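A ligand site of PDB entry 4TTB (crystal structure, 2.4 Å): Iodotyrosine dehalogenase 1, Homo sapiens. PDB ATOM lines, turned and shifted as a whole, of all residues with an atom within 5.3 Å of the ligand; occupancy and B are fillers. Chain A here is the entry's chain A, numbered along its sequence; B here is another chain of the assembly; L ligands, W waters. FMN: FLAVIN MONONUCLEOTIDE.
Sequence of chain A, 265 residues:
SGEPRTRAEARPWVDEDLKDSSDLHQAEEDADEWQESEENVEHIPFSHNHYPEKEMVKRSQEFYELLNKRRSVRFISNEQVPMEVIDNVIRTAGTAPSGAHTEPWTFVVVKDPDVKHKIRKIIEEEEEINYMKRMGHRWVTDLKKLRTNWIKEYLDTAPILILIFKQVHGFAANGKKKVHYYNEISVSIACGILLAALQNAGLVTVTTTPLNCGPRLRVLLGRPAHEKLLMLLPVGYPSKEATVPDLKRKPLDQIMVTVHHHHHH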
ATOM      1  N   ARG A  70      16.405 -13.416   5.446  1.00  0.00           N
ATOM      2  CA  ARG A  70      17.145 -12.715   4.429  1.00  0.00           C
ATOM      3  C   ARG A  70      16.966 -11.231   4.669  1.00  0.00           C
ATOM      4  O   ARG A  70      15.852 -10.763   4.885  1.00  0.00           O
ATOM      5  CB  ARG A  70      16.630 -13.065   3.037  1.00  0.00           C
ATOM      6  CG  ARG A  70      17.385 -12.358   1.928  1.00  0.00           C
ATOM      7  CD  ARG A  70      16.502 -12.152   0.711  1.00  0.00           C
ATOM      8  NE  ARG A  70      15.316 -11.380   1.056  1.00  0.00           N
ATOM      9  CZ  ARG A  70      15.306 -10.062   1.222  1.00  0.00           C
ATOM     10  NH1 ARG A  70      16.411  -9.344   1.056  1.00  0.00           N
ATOM     11  NH2 ARG A  70      14.174  -9.449   1.517  1.00  0.00           N
ATOM     12  N   ARG A  71      18.068 -10.484   4.632  1.00  0.00           N
ATOM     13  CA  ARG A  71      17.988  -9.030   4.719  1.00  0.00           C
ATOM     14  C   ARG A  71      18.959  -8.427   3.728  1.00  0.00           C
ATOM     15  O   ARG A  71      20.004  -9.012   3.460  1.00  0.00           O
ATOM     16  CB  ARG A  71      18.335  -8.550   6.136  1.00  0.00           C
ATOM     17  CG  ARG A  71      17.337  -8.974   7.220  1.00  0.00           C
ATOM     18  CD  ARG A  71      15.936  -8.453   6.912  1.00  0.00           C
ATOM     19  NE  ARG A  71      15.923  -7.013   6.690  1.00  0.00           N
ATOM     20  CZ  ARG A  71      15.882  -6.113   7.663  1.00  0.00           C
ATOM     21  NH1 ARG A  71      15.845  -6.516   8.930  1.00  0.00           N
ATOM     22  NH2 ARG A  71      15.875  -4.815   7.376  1.00  0.00           N
ATOM     23  N   SER A  72      18.614  -7.280   3.161  1.00  0.00           N
ATOM     24  CA  SER A  72      19.548  -6.557   2.319  1.00  0.00           C
ATOM     25  C   SER A  72      20.614  -6.006   3.247  1.00  0.00           C
ATOM     26  O   SER A  72      20.299  -5.267   4.182  1.00  0.00           O
ATOM     27  CB  SER A  72      18.850  -5.438   1.557  1.00  0.00           C
ATOM     28  OG  SER A  72      17.754  -5.969   0.826  1.00  0.00           O
ATOM     29  N   ARG A  74      24.147  -3.969   3.534  1.00  0.00           N
ATOM     30  CA  ARG A  74      24.930  -2.990   2.805  1.00  0.00           C
ATOM     31  C   ARG A  74      26.388  -2.981   3.206  1.00  0.00           C
ATOM     32  O   ARG A  74      27.152  -2.136   2.757  1.00  0.00           O
ATOM     33  CB  ARG A  74      24.268  -1.610   2.861  1.00  0.00           C
ATOM     34  CG  ARG A  74      22.922  -1.626   2.116  1.00  0.00           C
ATOM     35  CD  ARG A  74      21.983  -0.459   2.445  1.00  0.00           C
ATOM     36  NE  ARG A  74      20.706  -0.610   1.735  1.00  0.00           N
ATOM     37  CZ  ARG A  74      19.640  -1.252   2.221  1.00  0.00           C
ATOM     38  NH1 ARG A  74      19.679  -1.813   3.417  1.00  0.00           N
ATOM     39  NH2 ARG A  74      18.528  -1.353   1.502  1.00  0.00           N
ATOM     40  N   LYS A 152      28.349   4.253  -2.206  1.00  0.00           N
ATOM     41  CA  LYS A 152      28.195   2.810  -2.045  1.00  0.00           C
ATOM     42  C   LYS A 152      29.566   2.148  -2.001  1.00  0.00           C
ATOM     43  O   LYS A 152      30.144   1.846  -3.051  1.00  0.00           O
ATOM     44  CB  LYS A 152      27.462   2.260  -3.261  1.00  0.00           C
ATOM     45  CG  LYS A 152      26.245   3.074  -3.694  1.00  0.00           C
ATOM     46  CD  LYS A 152      25.167   3.041  -2.628  1.00  0.00           C
ATOM     47  CE  LYS A 152      23.775   3.253  -3.209  1.00  0.00           C
ATOM     48  NZ  LYS A 152      22.705   2.627  -2.362  1.00  0.00           N
ATOM     49  N   TYR A 154      30.257  -0.900  -0.784  1.00  0.00           N
ATOM     50  CA  TYR A 154      30.204  -2.341  -0.889  1.00  0.00           C
ATOM     51  C   TYR A 154      30.437  -2.855  -2.325  1.00  0.00           C
ATOM     52  O   TYR A 154      30.773  -4.019  -2.529  1.00  0.00           O
ATOM     53  CB  TYR A 154      28.894  -2.852  -0.302  1.00  0.00           C
ATOM     54  CG  TYR A 154      27.674  -2.117  -0.815  1.00  0.00           C
ATOM     55  CD1 TYR A 154      27.083  -1.112  -0.061  1.00  0.00           C
ATOM     56  CD2 TYR A 154      27.128  -2.423  -2.058  1.00  0.00           C
ATOM     57  CE1 TYR A 154      25.955  -0.446  -0.522  1.00  0.00           C
ATOM     58  CE2 TYR A 154      26.014  -1.747  -2.533  1.00  0.00           C
ATOM     59  CZ  TYR A 154      25.425  -0.765  -1.758  1.00  0.00           C
ATOM     60  OH  TYR A 154      24.317  -0.106  -2.233  1.00  0.00           O
ATOM     61  N   VAL A 206      22.684  -6.933  -1.540  1.00  0.00           N
ATOM     62  CA  VAL A 206      21.586  -5.983  -1.494  1.00  0.00           C
ATOM     63  C   VAL A 206      21.112  -5.765  -2.919  1.00  0.00           C
ATOM     64  O   VAL A 206      21.906  -5.435  -3.791  1.00  0.00           O
ATOM     65  CB  VAL A 206      21.983  -4.640  -0.815  1.00  0.00           C
ATOM     66  CG1 VAL A 206      23.320  -4.139  -1.330  1.00  0.00           C
ATOM     67  CG2 VAL A 206      20.901  -3.593  -1.029  1.00  0.00           C
ATOM     68  N   THR A 207      19.831  -6.022  -3.156  1.00  0.00           N
ATOM     69  CA  THR A 207      19.257  -5.878  -4.486  1.00  0.00           C
ATOM     70  C   THR A 207      19.304  -4.431  -4.926  1.00  0.00           C
ATOM     71  O   THR A 207      18.848  -3.559  -4.198  1.00  0.00           O
ATOM     72  CB  THR A 207      17.798  -6.311  -4.539  1.00  0.00           C
ATOM     73  OG1 THR A 207      17.668  -7.621  -3.980  1.00  0.00           O
ATOM     74  CG2 THR A 207      17.275  -6.307  -5.976  1.00  0.00           C
ATOM     75  N   THR A 208      19.859  -4.171  -6.095  1.00  0.00           N
ATOM     76  CA  THR A 208      19.825  -2.851  -6.688  1.00  0.00           C
ATOM     77  C   THR A 208      19.454  -2.964  -8.157  1.00  0.00           C
ATOM     78  O   THR A 208      19.860  -3.917  -8.837  1.00  0.00           O
ATOM     79  CB  THR A 208      21.168  -2.128  -6.563  1.00  0.00           C
ATOM     80  OG1 THR A 208      22.183  -2.895  -7.224  1.00  0.00           O
ATOM     81  CG2 THR A 208      21.570  -1.957  -5.114  1.00  0.00           C
ATOM     82  N   THR A 209      18.674  -2.010  -8.647  1.00  0.00           N
ATOM     83  CA  THR A 209      18.317  -1.980 -10.057  1.00  0.00           C
ATOM     84  C   THR A 209      18.728  -0.657 -10.694  1.00  0.00           C
ATOM     85  O   THR A 209      17.867   0.157 -11.046  1.00  0.00           O
ATOM     86  CB  THR A 209      16.812  -2.246 -10.265  1.00  0.00           C
ATOM     87  OG1 THR A 209      16.046  -1.202  -9.636  1.00  0.00           O
ATOM     88  CG2 THR A 209      16.419  -3.582  -9.664  1.00  0.00           C
ATOM     89  N   LEU A 247      13.183  -3.201  10.597  1.00  0.00           N
ATOM     90  CA  LEU A 247      12.005  -3.128   9.752  1.00  0.00           C
ATOM     91  C   LEU A 247      11.181  -4.359  10.032  1.00  0.00           C
ATOM     92  O   LEU A 247      11.714  -5.435  10.287  1.00  0.00           O
ATOM     93  CB  LEU A 247      12.382  -3.145   8.277  1.00  0.00           C
ATOM     94  CG  LEU A 247      13.231  -2.056   7.635  1.00  0.00           C
ATOM     95  CD1 LEU A 247      13.397  -2.361   6.136  1.00  0.00           C
ATOM     96  CD2 LEU A 247      12.603  -0.691   7.848  1.00  0.00           C
ATOM     97  N   ARG A 249       8.180  -7.007   8.534  1.00  0.00           N
ATOM     98  CA  ARG A 249       7.484  -7.414   7.342  1.00  0.00           C
ATOM     99  C   ARG A 249       6.018  -7.488   7.683  1.00  0.00           C
ATOM    100  O   ARG A 249       5.655  -7.774   8.822  1.00  0.00           O
ATOM    101  CB  ARG A 249       8.009  -8.730   6.809  1.00  0.00           C
ATOM    102  CG  ARG A 249       9.447  -8.645   6.440  1.00  0.00           C
ATOM    103  CD  ARG A 249       9.929  -9.822   5.653  1.00  0.00           C
ATOM    104  NE  ARG A 249      11.234  -9.518   5.077  1.00  0.00           N
ATOM    105  CZ  ARG A 249      12.339 -10.202   5.354  1.00  0.00           C
ATOM    106  NH1 ARG A 249      12.275 -11.227   6.188  1.00  0.00           N
ATOM    107  NH2 ARG A 249      13.476  -9.865   4.781  1.00  0.00           N
ATOM    108  N   THR B  95       8.589 -12.382   1.974  1.00  0.00           N
ATOM    109  CA  THR B  95       9.880 -12.069   2.559  1.00  0.00           C
ATOM    110  C   THR B  95      10.794 -11.417   1.539  1.00  0.00           C
ATOM    111  O   THR B  95      11.943 -11.074   1.844  1.00  0.00           O
ATOM    112  CB  THR B  95      10.614 -13.284   3.094  1.00  0.00           C
ATOM    113  OG1 THR B  95      11.257 -13.964   2.013  1.00  0.00           O
ATOM    114  CG2 THR B  95       9.680 -14.207   3.855  1.00  0.00           C
ATOM    115  N   ALA B  96      10.272 -11.233   0.338  1.00  0.00           N
ATOM    116  CA  ALA B  96      11.033 -10.633  -0.744  1.00  0.00           C
ATOM    117  C   ALA B  96      11.497  -9.207  -0.422  1.00  0.00           C
ATOM    118  O   ALA B  96      10.880  -8.500   0.376  1.00  0.00           O
ATOM    119  CB  ALA B  96      10.221 -10.664  -2.040  1.00  0.00           C
ATOM    120  N   PRO B  97      12.619  -8.790  -1.022  1.00  0.00           N
ATOM    121  CA  PRO B  97      13.026  -7.392  -0.936  1.00  0.00           C
ATOM    122  C   PRO B  97      12.097  -6.567  -1.807  1.00  0.00           C
ATOM    123  O   PRO B  97      11.579  -7.089  -2.791  1.00  0.00           O
ATOM    124  CB  PRO B  97      14.426  -7.409  -1.548  1.00  0.00           C
ATOM    125  CG  PRO B  97      14.405  -8.558  -2.498  1.00  0.00           C
ATOM    126  CD  PRO B  97      13.559  -9.604  -1.828  1.00  0.00           C
ATOM    127  N   SER B  98      11.838  -5.320  -1.452  1.00  0.00           N
ATOM    128  CA  SER B  98      11.083  -4.448  -2.331  1.00  0.00           C
ATOM    129  C   SER B  98      11.728  -3.073  -2.359  1.00  0.00           C
ATOM    130  O   SER B  98      12.384  -2.678  -1.395  1.00  0.00           O
ATOM    131  CB  SER B  98       9.592  -4.373  -1.954  1.00  0.00           C
ATOM    132  OG  SER B  98       9.397  -3.914  -0.631  1.00  0.00           O
ATOM    133  N   GLY B  99      11.575  -2.372  -3.472  1.00  0.00           N
ATOM    134  CA  GLY B  99      12.125  -1.033  -3.567  1.00  0.00           C
ATOM    135  C   GLY B  99      11.458  -0.112  -2.562  1.00  0.00           C
ATOM    136  O   GLY B  99      10.234   0.009  -2.566  1.00  0.00           O
ATOM    137  N   ALA B 100      12.261   0.527  -1.710  1.00  0.00           N
ATOM    138  CA  ALA B 100      11.753   1.394  -0.645  1.00  0.00           C
ATOM    139  C   ALA B 100      10.871   0.679   0.383  1.00  0.00           C
ATOM    140  O   ALA B 100      10.028   1.294   1.011  1.00  0.00           O
ATOM    141  CB  ALA B 100      10.996   2.596  -1.244  1.00  0.00           C
ATOM    142  N   HIS B 101      11.076  -0.636   0.534  1.00  0.00           N
ATOM    143  CA  HIS B 101      10.328  -1.424   1.521  1.00  0.00           C
ATOM    144  C   HIS B 101       8.794  -1.294   1.403  1.00  0.00           C
ATOM    145  O   HIS B 101       8.081  -1.371   2.408  1.00  0.00           O
ATOM    146  CB  HIS B 101      10.812  -1.071   2.933  1.00  0.00           C
ATOM    147  CG  HIS B 101      10.272  -1.959   4.010  1.00  0.00           C
ATOM    148  ND1 HIS B 101      10.153  -3.317   3.848  1.00  0.00           N
ATOM    149  CD2 HIS B 101       9.788  -1.678   5.246  1.00  0.00           C
ATOM    150  CE1 HIS B 101       9.636  -3.848   4.951  1.00  0.00           C
ATOM    151  NE2 HIS B 101       9.412  -2.870   5.807  1.00  0.00           N
ATOM    152  N   TYR B 182      10.250   0.352  -7.831  1.00  0.00           N
ATOM    153  CA  TYR B 182      10.230  -0.524  -9.003  1.00  0.00           C
ATOM    154  C   TYR B 182       9.300  -1.691  -8.726  1.00  0.00           C
ATOM    155  O   TYR B 182       9.743  -2.824  -8.573  1.00  0.00           O
ATOM    156  CB  TYR B 182      11.635  -1.042  -9.296  1.00  0.00           C
ATOM    157  CG  TYR B 182      12.647   0.059  -9.495  1.00  0.00           C
ATOM    158  CD1 TYR B 182      13.247   0.678  -8.402  1.00  0.00           C
ATOM    159  CD2 TYR B 182      12.999   0.492 -10.767  1.00  0.00           C
ATOM    160  CE1 TYR B 182      14.163   1.683  -8.568  1.00  0.00           C
ATOM    161  CE2 TYR B 182      13.915   1.497 -10.948  1.00  0.00           C
ATOM    162  CZ  TYR B 182      14.497   2.092  -9.841  1.00  0.00           C
ATOM    163  OH  TYR B 182      15.424   3.101 -10.015  1.00  0.00           O
ATOM    164  N   ILE B 185       9.287  -5.259 -10.881  1.00  0.00           N
ATOM    165  CA  ILE B 185      10.422  -6.103 -10.521  1.00  0.00           C
ATOM    166  C   ILE B 185      10.276  -6.667  -9.103  1.00  0.00           C
ATOM    167  O   ILE B 185      10.543  -7.848  -8.871  1.00  0.00           O
ATOM    168  CB  ILE B 185      11.735  -5.327 -10.658  1.00  0.00           C
ATOM    169  CG1 ILE B 185      11.893  -4.790 -12.069  1.00  0.00           C
ATOM    170  CG2 ILE B 185      12.922  -6.204 -10.297  1.00  0.00           C
ATOM    171  CD1 ILE B 185      13.196  -4.083 -12.292  1.00  0.00           C
ATOM    172  N   SER B 186       9.822  -5.838  -8.171  1.00  0.00           N
ATOM    173  CA  SER B 186       9.665  -6.279  -6.781  1.00  0.00           C
ATOM    174  C   SER B 186       8.655  -7.415  -6.689  1.00  0.00           C
ATOM    175  O   SER B 186       8.903  -8.434  -6.059  1.00  0.00           O
ATOM    176  CB  SER B 186       9.247  -5.119  -5.857  1.00  0.00           C
ATOM    177  OG  SER B 186      10.152  -4.015  -5.945  1.00  0.00           O
ATOM    178  N   ILE B 189      10.045 -10.532  -8.403  1.00  0.00           N
ATOM    179  CA  ILE B 189      11.020 -11.150  -7.500  1.00  0.00           C
ATOM    180  C   ILE B 189      10.305 -12.031  -6.491  1.00  0.00           C
ATOM    181  O   ILE B 189      10.677 -13.186  -6.312  1.00  0.00           O
ATOM    182  CB  ILE B 189      11.909 -10.133  -6.783  1.00  0.00           C
ATOM    183  CG1 ILE B 189      12.988  -9.582  -7.729  1.00  0.00           C
ATOM    184  CG2 ILE B 189      12.581 -10.755  -5.570  1.00  0.00           C
ATOM    185  CD1 ILE B 189      13.661  -8.305  -7.191  1.00  0.00           C
HETATM  186  N1  FMN L   1      18.420  -1.004  -1.559  1.00  0.00           N
HETATM  187  C2  FMN L   1      19.355   0.006  -1.570  1.00  0.00           C
HETATM  188  O2  FMN L   1      20.012   0.281  -0.579  1.00  0.00           O
HETATM  189  N3  FMN L   1      19.508   0.704  -2.738  1.00  0.00           N
HETATM  190  C4  FMN L   1      18.816   0.474  -3.913  1.00  0.00           C
HETATM  191  O4  FMN L   1      19.058   1.168  -4.881  1.00  0.00           O
HETATM  192  C4A FMN L   1      17.883  -0.560  -3.839  1.00  0.00           C
HETATM  193  N5  FMN L   1      17.185  -0.834  -4.931  1.00  0.00           N
HETATM  194  C5A FMN L   1      16.246  -1.857  -4.906  1.00  0.00           C
HETATM  195  C6  FMN L   1      15.494  -2.142  -6.070  1.00  0.00           C
HETATM  196  C7  FMN L   1      14.557  -3.158  -6.067  1.00  0.00           C
HETATM  197  C7M FMN L   1      13.796  -3.415  -7.336  1.00  0.00           C
HETATM  198  C8  FMN L   1      14.340  -3.924  -4.901  1.00  0.00           C
HETATM  199  C8M FMN L   1      13.310  -5.060  -4.874  1.00  0.00           C
HETATM  200  C9  FMN L   1      15.066  -3.653  -3.746  1.00  0.00           C
HETATM  201  C9A FMN L   1      16.033  -2.610  -3.755  1.00  0.00           C
HETATM  202  N10 FMN L   1      16.787  -2.288  -2.612  1.00  0.00           N
HETATM  203  C10 FMN L   1      17.702  -1.278  -2.686  1.00  0.00           C
HETATM  204  C1' FMN L   1      16.626  -3.037  -1.353  1.00  0.00           C
HETATM  205  C2' FMN L   1      15.492  -2.548  -0.486  1.00  0.00           C
HETATM  206  O2' FMN L   1      15.816  -1.305   0.098  1.00  0.00           O
HETATM  207  C3' FMN L   1      15.211  -3.605   0.631  1.00  0.00           C
HETATM  208  O3' FMN L   1      14.944  -4.837   0.049  1.00  0.00           O
HETATM  209  C4' FMN L   1      14.005  -3.180   1.466  1.00  0.00           C
HETATM  210  O4' FMN L   1      14.299  -1.989   2.134  1.00  0.00           O
HETATM  211  C5' FMN L   1      13.607  -4.248   2.460  1.00  0.00           C
HETATM  212  O5' FMN L   1      14.759  -4.630   3.223  1.00  0.00           O
HETATM  213  P   FMN L   1      15.219  -6.198   3.257  1.00  0.00           P
HETATM  214  O1P FMN L   1      16.454  -6.290   4.118  1.00  0.00           O
HETATM  215  O2P FMN L   1      15.532  -6.627   1.817  1.00  0.00           O
HETATM  216  O3P FMN L   1      14.093  -7.076   3.851  1.00  0.00           O
HETATM  217  O   HOH W   1      17.666  -4.078   5.199  1.00  0.00           O
HETATM  218  O   HOH W   2      15.322   1.360  -1.890  1.00  0.00           O
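Water W1 lies within hydrogen-bond range of an oxygen (O1P) of the ligand, the guanidinium group (NH2) of Arg 71 and the backbone carbonyl oxygen (O) of Ser 72.
Water W2 lies within hydrogen-bond range of N of Ala 100 of chain B (3.2 Å) and O2' of the ligand (3.4 Å).
O of Thr 207 lies close to N10 of the ligand.
Residues that only touch the ligand: Pro 97 of chain B, Gly 99 of chain B, Ser 186 of chain B, Thr 209, Val 206, His 101 of chain B, Lys 152, Thr 208, Tyr 182 of chain B and Leu 247.
Hydrophobic or aromatic side chains that line the ligand: Val 206, Leu 247, Pro 97 of chain B, His 101 of chain B and Tyr 182 of chain B.
The nearest printed residue that does not touch the ligand is Ile 189 of chain B (4.003 Å).
NH2 of Arg 249 lies within hydrogen-bond range of O of Arg 70, 2.5 Å away.
O of Thr 95 of chain B is in hydrogen-bond range of NH2 of Arg 70.
The side-chain hydroxyl (OG) of Ser 186 of chain B is in hydrogen-bond range of the backbone NH (N) of Gly 99 of chain B.
The side-chain hydroxyl of Ser 186 of chain B sits at hydrogen-bond distance from the backbone carbonyl oxygen of Tyr 182 of chain B.
The side-chain amino group (NZ) of Lys 152 is in hydrogen-bond range of the side-chain hydroxyl (OH) of Tyr 154, at 3.2 Å.
The backbone NH (N) of Ser 72 lies within hydrogen-bond range of an oxygen (O1P) of the ligand (2.6 Å).
An oxygen (O2P) of the ligand lies within hydrogen-bond range of the side-chain hydroxyl of Ser 72, 2.5 Å away.
The guanidinium group of Arg 74 lies within hydrogen-bond range of an oxygen (O2) of the ligand, at 2.6 Å.
NE of Arg 71 lies within salt-bridge range of O1P of the ligand (2.7 Å).
NH1 of Arg 70 is in salt-bridge range of O2P of the ligand, 3.0 Å away.
The guanidinium group of Arg 249 is in salt-bridge range of an oxygen (O3P) of the ligand.
An oxygen (O3') of the ligand is in hydrogen-bond range of the backbone NH (N) of Ser 98 of chain B, at 3.5 Å.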
